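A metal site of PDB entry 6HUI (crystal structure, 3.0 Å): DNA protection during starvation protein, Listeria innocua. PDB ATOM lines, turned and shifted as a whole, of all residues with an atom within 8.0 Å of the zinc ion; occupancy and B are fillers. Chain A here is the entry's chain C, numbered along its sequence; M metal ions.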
ATOM      1  N   PHE A  12      -8.316  10.774 -18.098  1.00  0.00           N
ATOM      2  CA  PHE A  12      -8.758  10.226 -16.817  1.00  0.00           C
ATOM      3  C   PHE A  12      -8.089   8.878 -16.538  1.00  0.00           C
ATOM      4  O   PHE A  12      -7.644   8.633 -15.415  1.00  0.00           O
ATOM      5  CB  PHE A  12     -10.281  10.093 -16.792  1.00  0.00           C
ATOM      6  CG  PHE A  12     -10.812   9.439 -15.560  1.00  0.00           C
ATOM      7  CD1 PHE A  12     -10.979  10.163 -14.392  1.00  0.00           C
ATOM      8  CD2 PHE A  12     -11.142   8.091 -15.550  1.00  0.00           C
ATOM      9  CE1 PHE A  12     -11.469   9.565 -13.245  1.00  0.00           C
ATOM     10  CE2 PHE A  12     -11.633   7.486 -14.411  1.00  0.00           C
ATOM     11  CZ  PHE A  12     -11.792   8.221 -13.257  1.00  0.00           C
ATOM     12  N   HIS A  15      -4.486   9.466 -15.644  1.00  0.00           N
ATOM     13  CA  HIS A  15      -4.484  10.048 -14.305  1.00  0.00           C
ATOM     14  C   HIS A  15      -4.642   8.964 -13.245  1.00  0.00           C
ATOM     15  O   HIS A  15      -3.916   8.936 -12.244  1.00  0.00           O
ATOM     16  CB  HIS A  15      -5.609  11.085 -14.203  1.00  0.00           C
ATOM     17  CG  HIS A  15      -5.543  11.932 -12.965  1.00  0.00           C
ATOM     18  ND1 HIS A  15      -4.377  12.135 -12.265  1.00  0.00           N
ATOM     19  CD2 HIS A  15      -6.498  12.635 -12.317  1.00  0.00           C
ATOM     20  CE1 HIS A  15      -4.629  12.920 -11.232  1.00  0.00           C
ATOM     21  NE2 HIS A  15      -5.909  13.239 -11.244  1.00  0.00           N
ATOM     22  N   GLN A  16      -5.593   8.047 -13.458  1.00  0.00           N
ATOM     23  CA  GLN A  16      -5.800   6.952 -12.516  1.00  0.00           C
ATOM     24  C   GLN A  16      -4.674   5.925 -12.569  1.00  0.00           C
ATOM     25  O   GLN A  16      -4.480   5.199 -11.589  1.00  0.00           O
ATOM     26  CB  GLN A  16      -7.134   6.268 -12.789  1.00  0.00           C
ATOM     27  CG  GLN A  16      -8.346   7.189 -12.631  1.00  0.00           C
ATOM     28  CD  GLN A  16      -8.450   7.790 -11.237  1.00  0.00           C
ATOM     29  OE1 GLN A  16      -7.986   7.214 -10.257  1.00  0.00           O
ATOM     30  NE2 GLN A  16      -9.064   8.965 -11.154  1.00  0.00           N
ATOM     31  N   ASN A  19      -2.289   7.635 -10.196  1.00  0.00           N
ATOM     32  CA  ASN A  19      -2.861   7.506  -8.858  1.00  0.00           C
ATOM     33  C   ASN A  19      -2.719   6.082  -8.324  1.00  0.00           C
ATOM     34  O   ASN A  19      -2.424   5.887  -7.144  1.00  0.00           O
ATOM     35  CB  ASN A  19      -4.339   7.903  -8.885  1.00  0.00           C
ATOM     36  CG  ASN A  19      -4.535   9.365  -9.195  1.00  0.00           C
ATOM     37  OD1 ASN A  19      -3.759  10.222  -8.763  1.00  0.00           O
ATOM     38  ND2 ASN A  19      -5.584   9.675  -9.952  1.00  0.00           N
ATOM     39  N   ASN A  81       1.768  13.713 -12.594  1.00  0.00           N
ATOM     40  CA  ASN A  81       0.346  13.743 -12.912  1.00  0.00           C
ATOM     41  C   ASN A  81      -0.557  13.163 -11.833  1.00  0.00           C
ATOM     42  O   ASN A  81      -1.781  13.338 -11.917  1.00  0.00           O
ATOM     43  CB  ASN A  81       0.075  12.996 -14.235  1.00  0.00           C
ATOM     44  CG  ASN A  81      -1.230  13.426 -14.893  1.00  0.00           C
ATOM     45  OD1 ASN A  81      -2.066  12.596 -15.224  1.00  0.00           O
ATOM     46  ND2 ASN A  81      -1.393  14.732 -15.074  1.00  0.00           N
ATOM     47  N   ALA A  82      -0.016  12.479 -10.830  1.00  0.00           N
ATOM     48  CA  ALA A  82      -0.870  11.862  -9.823  1.00  0.00           C
ATOM     49  C   ALA A  82      -1.463  12.908  -8.888  1.00  0.00           C
ATOM     50  O   ALA A  82      -0.810  13.888  -8.535  1.00  0.00           O
ATOM     51  CB  ALA A  82      -0.087  10.823  -9.014  1.00  0.00           C
ATOM     52  N   SER A  83      -2.717  12.690  -8.498  1.00  0.00           N
ATOM     53  CA  SER A  83      -3.387  13.526  -7.509  1.00  0.00           C
ATOM     54  C   SER A  83      -3.414  12.901  -6.123  1.00  0.00           C
ATOM     55  O   SER A  83      -4.000  13.485  -5.207  1.00  0.00           O
ATOM     56  CB  SER A  83      -4.816  13.846  -7.960  1.00  0.00           C
ATOM     57  OG  SER A  83      -5.565  12.653  -8.146  1.00  0.00           O
ATOM     58  N   VAL A  84      -2.810  11.729  -5.947  1.00  0.00           N
ATOM     59  CA  VAL A  84      -2.717  11.079  -4.641  1.00  0.00           C
ATOM     60  C   VAL A  84      -1.434  11.531  -3.971  1.00  0.00           C
ATOM     61  O   VAL A  84      -0.360  11.510  -4.579  1.00  0.00           O
ATOM     62  CB  VAL A  84      -2.763   9.552  -4.789  1.00  0.00           C
ATOM     63  CG1 VAL A  84      -2.571   8.876  -3.438  1.00  0.00           C
ATOM     64  CG2 VAL A  84      -4.073   9.111  -5.423  1.00  0.00           C
ATOM     65  N   LEU A 108     -10.596   9.111  -1.889  1.00  0.00           N
ATOM     66  CA  LEU A 108     -10.173   9.867  -3.069  1.00  0.00           C
ATOM     67  C   LEU A 108     -10.458   9.082  -4.347  1.00  0.00           C
ATOM     68  O   LEU A 108     -11.102   9.590  -5.269  1.00  0.00           O
ATOM     69  CB  LEU A 108      -8.691  10.211  -2.947  1.00  0.00           C
ATOM     70  CG  LEU A 108      -8.014  11.203  -3.901  1.00  0.00           C
ATOM     71  CD1 LEU A 108      -6.775  11.776  -3.241  1.00  0.00           C
ATOM     72  CD2 LEU A 108      -7.651  10.558  -5.220  1.00  0.00           C
ATOM     73  N   LEU A 109      -9.999   7.830  -4.394  1.00  0.00           N
ATOM     74  CA  LEU A 109     -10.246   7.006  -5.571  1.00  0.00           C
ATOM     75  C   LEU A 109     -11.735   6.721  -5.761  1.00  0.00           C
ATOM     76  O   LEU A 109     -12.193   6.519  -6.887  1.00  0.00           O
ATOM     77  CB  LEU A 109      -9.459   5.702  -5.485  1.00  0.00           C
ATOM     78  CG  LEU A 109      -7.934   5.849  -5.540  1.00  0.00           C
ATOM     79  CD1 LEU A 109      -7.265   4.487  -5.493  1.00  0.00           C
ATOM     80  CD2 LEU A 109      -7.513   6.617  -6.781  1.00  0.00           C
ATOM     81  N   GLU A 112     -13.087  10.104  -7.414  1.00  0.00           N
ATOM     82  CA  GLU A 112     -12.576  10.232  -8.772  1.00  0.00           C
ATOM     83  C   GLU A 112     -13.134   9.143  -9.689  1.00  0.00           C
ATOM     84  O   GLU A 112     -13.483   9.419 -10.847  1.00  0.00           O
ATOM     85  CB  GLU A 112     -11.051  10.200  -8.774  1.00  0.00           C
ATOM     86  CG  GLU A 112     -10.411  11.418  -8.127  1.00  0.00           C
ATOM     87  CD  GLU A 112      -9.056  11.740  -8.728  1.00  0.00           C
ATOM     88  OE1 GLU A 112      -8.675  11.097  -9.730  1.00  0.00           O
ATOM     89  OE2 GLU A 112      -8.367  12.640  -8.196  1.00  0.00           O
ATOM     90  N   GLN A 115     -16.602  10.140 -10.701  1.00  0.00           N
ATOM     91  CA  GLN A 115     -16.532  11.111 -11.787  1.00  0.00           C
ATOM     92  C   GLN A 115     -16.220  10.439 -13.113  1.00  0.00           C
ATOM     93  O   GLN A 115     -16.782  10.813 -14.154  1.00  0.00           O
ATOM     94  CB  GLN A 115     -15.487  12.188 -11.466  1.00  0.00           C
ATOM     95  CG  GLN A 115     -15.841  13.071 -10.285  1.00  0.00           C
ATOM     96  CD  GLN A 115     -14.779  14.110  -9.998  1.00  0.00           C
ATOM     97  OE1 GLN A 115     -13.704  14.104 -10.594  1.00  0.00           O
ATOM     98  NE2 GLN A 115     -15.080  15.021  -9.072  1.00  0.00           N
HETATM   99 ZN    ZN M   1      -7.224  13.950  -9.646  1.00  0.00          ZN
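The backbone carbonyl oxygen (O) of His 15 sits at hydrogen-bond distance from the side-chain amide nitrogen (ND2) of Asn 19 (2.9 Å).
ND1 of His 15 lies within hydrogen-bond range of O of Asn 81.
The side-chain amide nitrogen of Asn 19 sits at hydrogen-bond distance from the side-chain carboxylate of Glu 112.
NE2 of Gln 16 sits at hydrogen-bond distance from OE1 of Glu 112, at 2.6 Å.
The backbone NH of Ser 83 is in hydrogen-bond range of the side-chain amide oxygen of Asn 19.
NE2 of His 15 binds the zinc ion (2.2 Å).
The zinc ion is bound by OE2 of Glu 112 (2.3 Å).
The zinc ion is bound by the side-chain hydroxyl (OG) of Ser 83.
The zinc ion has three donor atoms within binding distance.
Of the 12 residues printed, 3 come within 4 Å of the zinc ion.
The nearest printed residue that does not touch the zinc ion is Asn 19 (4.6 Å).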
